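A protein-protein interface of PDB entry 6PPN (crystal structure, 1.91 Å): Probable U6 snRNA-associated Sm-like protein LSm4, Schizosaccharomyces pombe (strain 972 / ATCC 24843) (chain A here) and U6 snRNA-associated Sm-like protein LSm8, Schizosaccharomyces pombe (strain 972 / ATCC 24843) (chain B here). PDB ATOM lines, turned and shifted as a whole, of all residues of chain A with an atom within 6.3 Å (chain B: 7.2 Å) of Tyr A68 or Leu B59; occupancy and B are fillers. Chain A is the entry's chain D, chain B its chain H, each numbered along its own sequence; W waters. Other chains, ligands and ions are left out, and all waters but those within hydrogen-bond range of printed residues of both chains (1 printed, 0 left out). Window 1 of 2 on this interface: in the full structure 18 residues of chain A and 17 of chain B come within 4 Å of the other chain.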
ATOM      1  N   PRO A   3      -8.041  20.495 -21.156  1.00  0.00           N
ATOM      2  CA  PRO A   3      -6.692  20.894 -21.603  1.00  0.00           C
ATOM      3  C   PRO A   3      -5.775  19.717 -21.876  1.00  0.00           C
ATOM      4  O   PRO A   3      -5.036  19.726 -22.869  1.00  0.00           O
ATOM      5  CB  PRO A   3      -6.176  21.744 -20.429  1.00  0.00           C
ATOM      6  CG  PRO A   3      -7.409  22.308 -19.803  1.00  0.00           C
ATOM      7  CD  PRO A   3      -8.472  21.221 -19.953  1.00  0.00           C
ATOM      8  N   LEU A   4      -5.829  18.669 -21.050  1.00  0.00           N
ATOM      9  CA  LEU A   4      -4.960  17.527 -21.331  1.00  0.00           C
ATOM     10  C   LEU A   4      -5.444  16.756 -22.549  1.00  0.00           C
ATOM     11  O   LEU A   4      -4.643  16.116 -23.244  1.00  0.00           O
ATOM     12  CB  LEU A   4      -4.857  16.598 -20.131  1.00  0.00           C
ATOM     13  CG  LEU A   4      -4.021  17.053 -18.948  1.00  0.00           C
ATOM     14  CD1 LEU A   4      -3.831  15.846 -18.068  1.00  0.00           C
ATOM     15  CD2 LEU A   4      -2.684  17.631 -19.365  1.00  0.00           C
ATOM     16  N   LEU A   6      -6.488  18.257 -25.249  1.00  0.00           N
ATOM     17  CA  LEU A   6      -5.825  18.993 -26.321  1.00  0.00           C
ATOM     18  C   LEU A   6      -4.335  18.680 -26.369  1.00  0.00           C
ATOM     19  O   LEU A   6      -3.766  18.430 -27.442  1.00  0.00           O
ATOM     20  CB  LEU A   6      -6.023  20.494 -26.104  1.00  0.00           C
ATOM     21  CG  LEU A   6      -6.067  21.484 -27.276  1.00  0.00           C
ATOM     22  CD1 LEU A   6      -5.323  22.769 -26.947  1.00  0.00           C
ATOM     23  CD2 LEU A   6      -5.604  20.886 -28.557  1.00  0.00           C
ATOM     24  N   LEU A   7      -3.700  18.623 -25.201  1.00  0.00           N
ATOM     25  CA  LEU A   7      -2.264  18.402 -25.175  1.00  0.00           C
ATOM     26  C   LEU A   7      -1.945  17.029 -25.734  1.00  0.00           C
ATOM     27  O   LEU A   7      -1.088  16.896 -26.613  1.00  0.00           O
ATOM     28  CB  LEU A   7      -1.745  18.619 -23.757  1.00  0.00           C
ATOM     29  CG  LEU A   7      -0.300  18.850 -23.306  1.00  0.00           C
ATOM     30  CD1 LEU A   7       0.168  17.767 -22.341  1.00  0.00           C
ATOM     31  CD2 LEU A   7       0.698  19.117 -24.417  1.00  0.00           C
ATOM     32  N   LEU A  16       5.124  25.075 -28.893  1.00  0.00           N
ATOM     33  CA  LEU A  16       5.987  26.042 -28.237  1.00  0.00           C
ATOM     34  C   LEU A  16       5.689  26.030 -26.742  1.00  0.00           C
ATOM     35  O   LEU A  16       4.526  26.074 -26.340  1.00  0.00           O
ATOM     36  CB  LEU A  16       5.770  27.440 -28.833  1.00  0.00           C
ATOM     37  CG  LEU A  16       6.706  28.549 -28.314  1.00  0.00           C
ATOM     38  CD1 LEU A  16       6.963  29.481 -29.427  1.00  0.00           C
ATOM     39  CD2 LEU A  16       6.089  29.316 -27.198  1.00  0.00           C
ATOM     40  N   VAL A  17       6.730  25.937 -25.916  1.00  0.00           N
ATOM     41  CA  VAL A  17       6.599  25.820 -24.467  1.00  0.00           C
ATOM     42  C   VAL A  17       7.320  26.992 -23.830  1.00  0.00           C
ATOM     43  O   VAL A  17       8.485  27.250 -24.152  1.00  0.00           O
ATOM     44  CB  VAL A  17       7.214  24.504 -23.951  1.00  0.00           C
ATOM     45  CG1 VAL A  17       6.956  24.343 -22.436  1.00  0.00           C
ATOM     46  CG2 VAL A  17       6.661  23.345 -24.706  1.00  0.00           C
ATOM     47  N   GLU A  18       6.670  27.692 -22.907  1.00  0.00           N
ATOM     48  CA  GLU A  18       7.403  28.680 -22.133  1.00  0.00           C
ATOM     49  C   GLU A  18       7.372  28.291 -20.662  1.00  0.00           C
ATOM     50  O   GLU A  18       6.286  28.068 -20.093  1.00  0.00           O
ATOM     51  CB  GLU A  18       6.870  30.103 -22.303  1.00  0.00           C
ATOM     52  CG  GLU A  18       7.838  31.115 -21.632  1.00  0.00           C
ATOM     53  CD  GLU A  18       7.460  32.570 -21.805  1.00  0.00           C
ATOM     54  OE1 GLU A  18       7.704  33.349 -20.855  1.00  0.00           O
ATOM     55  OE2 GLU A  18       6.920  32.942 -22.867  1.00  0.00           O
ATOM     56  N   LEU A  19       8.557  28.284 -20.043  1.00  0.00           N
ATOM     57  CA  LEU A  19       8.756  27.869 -18.653  1.00  0.00           C
ATOM     58  C   LEU A  19       8.729  29.052 -17.711  1.00  0.00           C
ATOM     59  O   LEU A  19       8.949  30.193 -18.117  1.00  0.00           O
ATOM     60  CB  LEU A  19      10.117  27.185 -18.499  1.00  0.00           C
ATOM     61  CG  LEU A  19      10.505  26.004 -19.387  1.00  0.00           C
ATOM     62  CD1 LEU A  19      11.849  25.505 -18.862  1.00  0.00           C
ATOM     63  CD2 LEU A  19       9.443  24.913 -19.277  1.00  0.00           C
ATOM     64  N   THR A  24      12.148  29.453 -23.566  1.00  0.00           N
ATOM     65  CA  THR A  24      11.140  28.867 -24.426  1.00  0.00           C
ATOM     66  C   THR A  24      11.758  27.685 -25.151  1.00  0.00           C
ATOM     67  O   THR A  24      12.959  27.676 -25.432  1.00  0.00           O
ATOM     68  CB  THR A  24      10.632  29.854 -25.482  1.00  0.00           C
ATOM     69  OG1 THR A  24      11.706  30.123 -26.369  1.00  0.00           O
ATOM     70  CG2 THR A  24      10.266  31.142 -24.829  1.00  0.00           C
ATOM     71  N   MET A  36       1.639  16.890 -17.062  1.00  0.00           N
ATOM     72  CA  MET A  36       2.052  17.844 -18.078  1.00  0.00           C
ATOM     73  C   MET A  36       3.561  17.772 -18.281  1.00  0.00           C
ATOM     74  O   MET A  36       4.153  18.680 -18.908  1.00  0.00           O
ATOM     75  CB  MET A  36       1.576  19.268 -17.760  1.00  0.00           C
ATOM     76  CG  MET A  36       1.304  20.149 -18.985  1.00  0.00           C
ATOM     77  SD  MET A  36       0.744  21.828 -18.514  1.00  0.00           S
ATOM     78  CE  MET A  36      -0.933  21.455 -18.147  1.00  0.00           C
ATOM     79  N   ILE A  66       6.068  24.617 -16.351  1.00  0.00           N
ATOM     80  CA  ILE A  66       5.509  25.191 -17.571  1.00  0.00           C
ATOM     81  C   ILE A  66       4.633  26.368 -17.190  1.00  0.00           C
ATOM     82  O   ILE A  66       3.841  26.281 -16.247  1.00  0.00           O
ATOM     83  CB  ILE A  66       4.675  24.142 -18.317  1.00  0.00           C
ATOM     84  CG1 ILE A  66       5.554  23.040 -18.884  1.00  0.00           C
ATOM     85  CG2 ILE A  66       3.843  24.795 -19.428  1.00  0.00           C
ATOM     86  CD1 ILE A  66       4.719  21.974 -19.601  1.00  0.00           C
ATOM     87  N   LYS A  67       4.769  27.476 -17.911  1.00  0.00           N
ATOM     88  CA  LYS A  67       3.790  28.557 -17.811  1.00  0.00           C
ATOM     89  C   LYS A  67       2.707  28.355 -18.859  1.00  0.00           C
ATOM     90  O   LYS A  67       1.509  28.321 -18.531  1.00  0.00           O
ATOM     91  CB  LYS A  67       4.485  29.914 -17.975  1.00  0.00           C
ATOM     92  CG  LYS A  67       4.484  30.741 -16.717  1.00  0.00           C
ATOM     93  CD  LYS A  67       5.707  31.606 -16.618  1.00  0.00           C
ATOM     94  CE  LYS A  67       5.973  32.264 -17.932  1.00  0.00           C
ATOM     95  NZ  LYS A  67       6.923  33.378 -17.792  1.00  0.00           N
ATOM     96  N   TYR A  68       3.101  28.175 -20.115  1.00  0.00           N
ATOM     97  CA  TYR A  68       2.045  27.925 -21.090  1.00  0.00           C
ATOM     98  C   TYR A  68       2.609  27.206 -22.301  1.00  0.00           C
ATOM     99  O   TYR A  68       3.821  27.137 -22.498  1.00  0.00           O
ATOM    100  CB  TYR A  68       1.365  29.224 -21.511  1.00  0.00           C
ATOM    101  CG  TYR A  68       2.315  30.104 -22.232  1.00  0.00           C
ATOM    102  CD1 TYR A  68       3.032  31.089 -21.565  1.00  0.00           C
ATOM    103  CD2 TYR A  68       2.537  29.924 -23.595  1.00  0.00           C
ATOM    104  CE1 TYR A  68       3.942  31.878 -22.264  1.00  0.00           C
ATOM    105  CE2 TYR A  68       3.431  30.702 -24.294  1.00  0.00           C
ATOM    106  CZ  TYR A  68       4.128  31.669 -23.640  1.00  0.00           C
ATOM    107  OH  TYR A  68       5.006  32.414 -24.390  1.00  0.00           O
ATOM    108  N   LEU A  69       1.693  26.656 -23.110  1.00  0.00           N
ATOM    109  CA  LEU A  69       1.989  25.995 -24.366  1.00  0.00           C
ATOM    110  C   LEU A  69       1.218  26.663 -25.487  1.00  0.00           C
ATOM    111  O   LEU A  69       0.063  27.038 -25.304  1.00  0.00           O
ATOM    112  CB  LEU A  69       1.592  24.525 -24.330  1.00  0.00           C
ATOM    113  CG  LEU A  69       2.052  23.901 -23.016  1.00  0.00           C
ATOM    114  CD1 LEU A  69       1.116  22.822 -22.635  1.00  0.00           C
ATOM    115  CD2 LEU A  69       3.400  23.337 -23.224  1.00  0.00           C
ATOM    116  N   ARG A  70       1.826  26.732 -26.669  1.00  0.00           N
ATOM    117  CA  ARG A  70       1.171  27.249 -27.856  1.00  0.00           C
ATOM    118  C   ARG A  70       1.067  26.099 -28.824  1.00  0.00           C
ATOM    119  O   ARG A  70       2.047  25.368 -29.027  1.00  0.00           O
ATOM    120  CB  ARG A  70       1.937  28.400 -28.483  1.00  0.00           C
ATOM    121  CG  ARG A  70       1.866  29.659 -27.647  1.00  0.00           C
ATOM    122  CD  ARG A  70       2.527  30.839 -28.346  1.00  0.00           C
ATOM    123  NE  ARG A  70       1.934  31.062 -29.653  1.00  0.00           N
ATOM    124  CZ  ARG A  70       2.387  31.960 -30.517  1.00  0.00           C
ATOM    125  NH1 ARG A  70       3.443  32.692 -30.188  1.00  0.00           N
ATOM    126  NH2 ARG A  70       1.796  32.117 -31.697  1.00  0.00           N
ATOM    127  N   ILE A  71      -0.127  25.940 -29.401  1.00  0.00           N
ATOM    128  CA  ILE A  71      -0.537  24.766 -30.156  1.00  0.00           C
ATOM    129  C   ILE A  71      -1.207  25.253 -31.427  1.00  0.00           C
ATOM    130  O   ILE A  71      -1.862  26.303 -31.434  1.00  0.00           O
ATOM    131  CB  ILE A  71      -1.490  23.892 -29.312  1.00  0.00           C
ATOM    132  CG1 ILE A  71      -0.711  23.315 -28.130  1.00  0.00           C
ATOM    133  CG2 ILE A  71      -2.060  22.765 -30.096  1.00  0.00           C
ATOM    134  CD1 ILE A  71      -1.565  22.967 -26.975  1.00  0.00           C
ATOM    135  N   THR B  15      -2.114  36.528 -15.563  1.00  0.00           N
ATOM    136  CA  THR B  15      -1.237  35.464 -15.108  1.00  0.00           C
ATOM    137  C   THR B  15      -0.334  35.954 -13.986  1.00  0.00           C
ATOM    138  O   THR B  15      -0.265  37.154 -13.675  1.00  0.00           O
ATOM    139  CB  THR B  15      -0.400  34.949 -16.273  1.00  0.00           C
ATOM    140  OG1 THR B  15       0.339  36.027 -16.809  1.00  0.00           O
ATOM    141  CG2 THR B  15      -1.276  34.472 -17.366  1.00  0.00           C
ATOM    142  N   ASP B  17       2.798  36.228 -13.832  1.00  0.00           N
ATOM    143  CA  ASP B  17       3.865  37.117 -14.268  1.00  0.00           C
ATOM    144  C   ASP B  17       3.325  38.438 -14.791  1.00  0.00           C
ATOM    145  O   ASP B  17       4.083  39.211 -15.387  1.00  0.00           O
ATOM    146  CB  ASP B  17       4.746  36.447 -15.336  1.00  0.00           C
ATOM    147  CG  ASP B  17       3.937  35.838 -16.475  1.00  0.00           C
ATOM    148  OD1 ASP B  17       2.713  36.065 -16.528  1.00  0.00           O
ATOM    149  OD2 ASP B  17       4.527  35.138 -17.339  1.00  0.00           O
ATOM    150  N   ARG B  19       0.965  39.151 -17.065  1.00  0.00           N
ATOM    151  CA  ARG B  19       0.590  39.331 -18.455  1.00  0.00           C
ATOM    152  C   ARG B  19      -0.926  39.289 -18.580  1.00  0.00           C
ATOM    153  O   ARG B  19      -1.622  38.750 -17.727  1.00  0.00           O
ATOM    154  CB  ARG B  19       1.215  38.250 -19.352  1.00  0.00           C
ATOM    155  CG  ARG B  19       2.651  38.512 -19.714  1.00  0.00           C
ATOM    156  CD  ARG B  19       3.582  37.378 -19.390  1.00  0.00           C
ATOM    157  NE  ARG B  19       3.713  36.345 -20.417  1.00  0.00           N
ATOM    158  CZ  ARG B  19       4.885  35.859 -20.830  1.00  0.00           C
ATOM    159  NH1 ARG B  19       4.928  34.912 -21.751  1.00  0.00           N
ATOM    160  NH2 ARG B  19       6.023  36.335 -20.334  1.00  0.00           N
ATOM    161  N   ASP B  29      -9.819  22.750 -16.434  1.00  0.00           N
ATOM    162  CA  ASP B  29      -9.982  21.585 -15.571  1.00  0.00           C
ATOM    163  C   ASP B  29      -9.800  22.014 -14.113  1.00  0.00           C
ATOM    164  O   ASP B  29      -9.605  23.194 -13.799  1.00  0.00           O
ATOM    165  CB  ASP B  29      -9.004  20.473 -15.982  1.00  0.00           C
ATOM    166  CG  ASP B  29      -7.560  20.925 -15.906  1.00  0.00           C
ATOM    167  OD1 ASP B  29      -7.264  21.735 -15.023  1.00  0.00           O
ATOM    168  OD2 ASP B  29      -6.706  20.498 -16.717  1.00  0.00           O
ATOM    169  N   ASN B  33      -5.977  24.781 -15.346  1.00  0.00           N
ATOM    170  CA  ASN B  33      -5.463  24.790 -16.714  1.00  0.00           C
ATOM    171  C   ASN B  33      -6.558  25.362 -17.607  1.00  0.00           C
ATOM    172  O   ASN B  33      -7.739  25.157 -17.350  1.00  0.00           O
ATOM    173  CB  ASN B  33      -5.096  23.376 -17.196  1.00  0.00           C
ATOM    174  CG  ASN B  33      -3.951  22.737 -16.404  1.00  0.00           C
ATOM    175  OD1 ASN B  33      -3.038  23.417 -15.926  1.00  0.00           O
ATOM    176  ND2 ASN B  33      -4.019  21.404 -16.238  1.00  0.00           N
ATOM    177  N   LEU B  34      -6.179  26.134 -18.618  1.00  0.00           N
ATOM    178  CA  LEU B  34      -7.169  26.752 -19.497  1.00  0.00           C
ATOM    179  C   LEU B  34      -6.751  26.544 -20.942  1.00  0.00           C
ATOM    180  O   LEU B  34      -5.559  26.477 -21.241  1.00  0.00           O
ATOM    181  CB  LEU B  34      -7.309  28.258 -19.262  1.00  0.00           C
ATOM    182  CG  LEU B  34      -7.473  28.745 -17.832  1.00  0.00           C
ATOM    183  CD1 LEU B  34      -7.396  30.259 -17.834  1.00  0.00           C
ATOM    184  CD2 LEU B  34      -8.804  28.296 -17.252  1.00  0.00           C
ATOM    185  N   ILE B  35      -7.741  26.452 -21.840  1.00  0.00           N
ATOM    186  CA  ILE B  35      -7.521  26.571 -23.278  1.00  0.00           C
ATOM    187  C   ILE B  35      -8.166  27.873 -23.733  1.00  0.00           C
ATOM    188  O   ILE B  35      -9.386  28.039 -23.610  1.00  0.00           O
ATOM    189  CB  ILE B  35      -8.138  25.403 -24.063  1.00  0.00           C
ATOM    190  CG1 ILE B  35      -7.615  24.052 -23.595  1.00  0.00           C
ATOM    191  CG2 ILE B  35      -7.863  25.580 -25.562  1.00  0.00           C
ATOM    192  CD1 ILE B  35      -8.473  22.882 -24.120  1.00  0.00           C
ATOM    193  N   LEU B  36      -7.383  28.744 -24.356  1.00  0.00           N
ATOM    194  CA  LEU B  36      -7.909  29.918 -25.037  1.00  0.00           C
ATOM    195  C   LEU B  36      -7.632  29.781 -26.527  1.00  0.00           C
ATOM    196  O   LEU B  36      -6.548  29.351 -26.922  1.00  0.00           O
ATOM    197  CB  LEU B  36      -7.243  31.190 -24.533  1.00  0.00           C
ATOM    198  CG  LEU B  36      -7.260  31.398 -23.032  1.00  0.00           C
ATOM    199  CD1 LEU B  36      -6.708  32.773 -22.718  1.00  0.00           C
ATOM    200  CD2 LEU B  36      -8.638  31.255 -22.559  1.00  0.00           C
ATOM    201  N   SER B  39      -6.564  33.816 -29.298  1.00  0.00           N
ATOM    202  CA  SER B  39      -6.111  34.640 -28.193  1.00  0.00           C
ATOM    203  C   SER B  39      -5.047  35.641 -28.638  1.00  0.00           C
ATOM    204  O   SER B  39      -4.418  35.524 -29.696  1.00  0.00           O
ATOM    205  CB  SER B  39      -5.531  33.778 -27.087  1.00  0.00           C
ATOM    206  OG  SER B  39      -4.378  33.161 -27.597  1.00  0.00           O
ATOM    207  N   GLU B  41      -2.178  38.722 -26.632  1.00  0.00           N
ATOM    208  CA  GLU B  41      -1.722  39.369 -25.411  1.00  0.00           C
ATOM    209  C   GLU B  41      -1.871  40.864 -25.588  1.00  0.00           C
ATOM    210  O   GLU B  41      -1.660  41.374 -26.683  1.00  0.00           O
ATOM    211  CB  GLU B  41      -0.265  39.042 -25.093  1.00  0.00           C
ATOM    212  CG  GLU B  41       0.259  39.870 -23.941  1.00  0.00           C
ATOM    213  CD  GLU B  41       1.606  39.414 -23.411  1.00  0.00           C
ATOM    214  OE1 GLU B  41       1.992  39.893 -22.324  1.00  0.00           O
ATOM    215  OE2 GLU B  41       2.264  38.573 -24.059  1.00  0.00           O
ATOM    216  N   LEU B  55      -1.602  35.283 -30.464  1.00  0.00           N
ATOM    217  CA  LEU B  55      -1.098  34.062 -29.851  1.00  0.00           C
ATOM    218  C   LEU B  55      -1.752  32.766 -30.337  1.00  0.00           C
ATOM    219  O   LEU B  55      -1.210  31.689 -30.065  1.00  0.00           O
ATOM    220  CB  LEU B  55      -1.242  34.145 -28.325  1.00  0.00           C
ATOM    221  CG  LEU B  55      -0.442  35.239 -27.604  1.00  0.00           C
ATOM    222  CD1 LEU B  55      -0.687  35.134 -26.088  1.00  0.00           C
ATOM    223  CD2 LEU B  55       1.007  35.079 -27.902  1.00  0.00           C
ATOM    224  N   GLY B  56      -2.896  32.821 -31.012  1.00  0.00           N
ATOM    225  CA  GLY B  56      -3.480  31.586 -31.512  1.00  0.00           C
ATOM    226  C   GLY B  56      -4.076  30.788 -30.370  1.00  0.00           C
ATOM    227  O   GLY B  56      -4.759  31.329 -29.492  1.00  0.00           O
ATOM    228  N   VAL B  57      -3.828  29.472 -30.373  1.00  0.00           N
ATOM    229  CA  VAL B  57      -4.302  28.597 -29.304  1.00  0.00           C
ATOM    230  C   VAL B  57      -3.266  28.568 -28.196  1.00  0.00           C
ATOM    231  O   VAL B  57      -2.080  28.319 -28.447  1.00  0.00           O
ATOM    232  CB  VAL B  57      -4.575  27.177 -29.822  1.00  0.00           C
ATOM    233  CG1 VAL B  57      -5.148  26.355 -28.708  1.00  0.00           C
ATOM    234  CG2 VAL B  57      -5.524  27.192 -31.031  1.00  0.00           C
ATOM    235  N   TYR B  58      -3.732  28.775 -26.972  1.00  0.00           N
ATOM    236  CA  TYR B  58      -2.906  29.037 -25.797  1.00  0.00           C
ATOM    237  C   TYR B  58      -3.375  28.119 -24.695  1.00  0.00           C
ATOM    238  O   TYR B  58      -4.533  28.206 -24.289  1.00  0.00           O
ATOM    239  CB  TYR B  58      -3.062  30.477 -25.340  1.00  0.00           C
ATOM    240  CG  TYR B  58      -1.800  31.146 -24.890  1.00  0.00           C
ATOM    241  CD1 TYR B  58      -0.717  31.236 -25.731  1.00  0.00           C
ATOM    242  CD2 TYR B  58      -1.720  31.743 -23.638  1.00  0.00           C
ATOM    243  CE1 TYR B  58       0.431  31.877 -25.346  1.00  0.00           C
ATOM    244  CE2 TYR B  58      -0.568  32.392 -23.241  1.00  0.00           C
ATOM    245  CZ  TYR B  58       0.502  32.445 -24.099  1.00  0.00           C
ATOM    246  OH  TYR B  58       1.656  33.090 -23.719  1.00  0.00           O
ATOM    247  N   LEU B  59      -2.535  27.185 -24.272  1.00  0.00           N
ATOM    248  CA  LEU B  59      -2.833  26.370 -23.101  1.00  0.00           C
ATOM    249  C   LEU B  59      -2.079  26.945 -21.901  1.00  0.00           C
ATOM    250  O   LEU B  59      -0.848  27.003 -21.908  1.00  0.00           O
ATOM    251  CB  LEU B  59      -2.448  24.913 -23.356  1.00  0.00           C
ATOM    252  CG  LEU B  59      -3.176  23.832 -22.559  1.00  0.00           C
ATOM    253  CD1 LEU B  59      -2.856  22.518 -23.186  1.00  0.00           C
ATOM    254  CD2 LEU B  59      -2.792  23.826 -21.082  1.00  0.00           C
ATOM    255  N   LEU B  60      -2.797  27.381 -20.883  1.00  0.00           N
ATOM    256  CA  LEU B  60      -2.174  28.035 -19.739  1.00  0.00           C
ATOM    257  C   LEU B  60      -2.220  27.062 -18.571  1.00  0.00           C
ATOM    258  O   LEU B  60      -3.283  26.512 -18.261  1.00  0.00           O
ATOM    259  CB  LEU B  60      -2.900  29.316 -19.332  1.00  0.00           C
ATOM    260  CG  LEU B  60      -2.757  30.531 -20.245  1.00  0.00           C
ATOM    261  CD1 LEU B  60      -3.988  30.690 -21.132  1.00  0.00           C
ATOM    262  CD2 LEU B  60      -2.492  31.789 -19.433  1.00  0.00           C
ATOM    263  N   ARG B  61      -1.079  26.838 -17.933  1.00  0.00           N
ATOM    264  CA  ARG B  61      -1.051  25.950 -16.781  1.00  0.00           C
ATOM    265  C   ARG B  61      -1.648  26.690 -15.594  1.00  0.00           C
ATOM    266  O   ARG B  61      -1.283  27.841 -15.342  1.00  0.00           O
ATOM    267  CB  ARG B  61       0.375  25.505 -16.495  1.00  0.00           C
ATOM    268  CG  ARG B  61       0.523  24.548 -15.306  1.00  0.00           C
ATOM    269  CD  ARG B  61       1.956  23.979 -15.242  1.00  0.00           C
ATOM    270  NE  ARG B  61       2.193  23.303 -13.970  1.00  0.00           N
ATOM    271  CZ  ARG B  61       1.924  22.015 -13.748  1.00  0.00           C
ATOM    272  NH1 ARG B  61       1.420  21.246 -14.716  1.00  0.00           N
ATOM    273  NH2 ARG B  61       2.175  21.488 -12.560  1.00  0.00           N
ATOM    274  N   GLY B  62      -2.554  26.027 -14.859  1.00  0.00           N
ATOM    275  CA  GLY B  62      -3.368  26.726 -13.859  1.00  0.00           C
ATOM    276  C   GLY B  62      -2.566  27.384 -12.750  1.00  0.00           C
ATOM    277  O   GLY B  62      -2.932  28.448 -12.235  1.00  0.00           O
ATOM    278  N   ASN B  64      -0.269  29.136 -13.036  1.00  0.00           N
ATOM    279  CA  ASN B  64       0.214  30.439 -13.464  1.00  0.00           C
ATOM    280  C   ASN B  64      -0.936  31.411 -13.673  1.00  0.00           C
ATOM    281  O   ASN B  64      -0.711  32.578 -14.010  1.00  0.00           O
ATOM    282  CB  ASN B  64       1.077  30.250 -14.727  1.00  0.00           C
ATOM    283  CG  ASN B  64       1.664  31.563 -15.267  1.00  0.00           C
ATOM    284  OD1 ASN B  64       1.391  31.929 -16.411  1.00  0.00           O
ATOM    285  ND2 ASN B  64       2.480  32.259 -14.466  1.00  0.00           N
HETATM  286  O   HOH W   1      -7.312  18.671 -18.573  1.00  0.00           O
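The side-chain carboxylate (OE2) of Glu A18 is in salt-bridge range of the guanidinium group (NH1) of Arg B19, at 3.0 Å.
The side-chain amino group of Lys A67 lies within salt-bridge range of the side-chain carboxylate of Asp B17, at 3.0 Å.
The backbone carbonyl oxygen (O) of Lys A67 lies within hydrogen-bond range of the backbone NH (N) of Arg B61 (3.0 Å).
The side-chain hydroxyl (OH) of Tyr A68 lies close to the side-chain hydroxyl (OH) of Tyr B58, 3.5 Å away.
The backbone carbonyl oxygen (O) of Leu A69 sits at hydrogen-bond distance from the backbone NH (N) of Leu B59.
The guanidinium group (NE) of Arg A70 is in hydrogen-bond range of the backbone carbonyl oxygen (O) of Leu B55.
The backbone carbonyl oxygen (O) of Val B57 sits at hydrogen-bond distance from the backbone NH (N) of Ile A71 (3.2 Å).
The backbone carbonyl oxygen (O) of Leu A16 sits at hydrogen-bond distance from the backbone NH (N) of Arg A70 (2.8 Å).
NZ of Lys A67 lies within salt-bridge range of OE1 of Glu A18.
OE2 of Glu A18 lies within hydrogen-bond range of OH of Tyr A68, 2.5 Å away.
OG1 of Thr B15 lies within hydrogen-bond range of N of Arg B19.
The backbone NH of Gly B62 sits at hydrogen-bond distance from the side-chain amide oxygen of Asn B33.
N of Leu B55 lies within hydrogen-bond range of O of Ser B39, at 2.9 Å.
CA of Pro A3 touches CD1 of Ile B35 (3.7 Å).
Pro A3 touches Leu B59 (O to CD1, 3.6 Å).
CB of Leu A6 touches CD1 of Ile B35, at 3.95 Å.
NH1 of Arg B61 touches CB of Met A36 (3.6 Å).
Ile A66 touches Arg B61.
CA of Leu B60 touches O of Lys A67, 3.9 Å away.
Arg B19 touches Tyr A68 (NH1 to CE1, 3.2 Å).
Leu B59 touches Tyr A68.
Arg A70 touches Val B57.
Arg A70 touches Tyr B58.
Tyr A68 touches just these residues of chain B: Arg B19 (3.2 Å), Tyr B58 (2.9 Å) and Leu B59 (3.1 Å).
Of chain A, only Pro A3 (3.6 Å), Tyr A68 (3.1 Å) and Leu A69 (2.8 Å) come within 4 Å of Leu B59.
Of the printed residues of chain A, Asp B29 touches Pro A3 (3.6 Å).
Of the printed residues of chain B, Ile A66 touches Arg B61 (3.1 Å).
Of the printed residues of chain A, Leu B55 touches Arg A70.
Printed residues of chain B within 4 Å of Pro A3: Asp B29, Asn B33, Ile B35 and Leu B59.
Ser B39 touches none of the printed residues of chain A.
Thr B15 touches none of the printed residues of chain A.
The nearest residue of chain A that does not touch Leu B59 is Ile A71 (4.03 Å).
The nearest printed residue of chain A that does not touch Tyr B58 is Ile A71 (5.2 Å).
Among the printed residues, 23 pairs touch across the chains.
Water W1 bridges the side-chain carboxylate (OD2) of Asp B29 (2.7 Å) and the backbone NH (N) of Leu A4 (2.9 Å).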
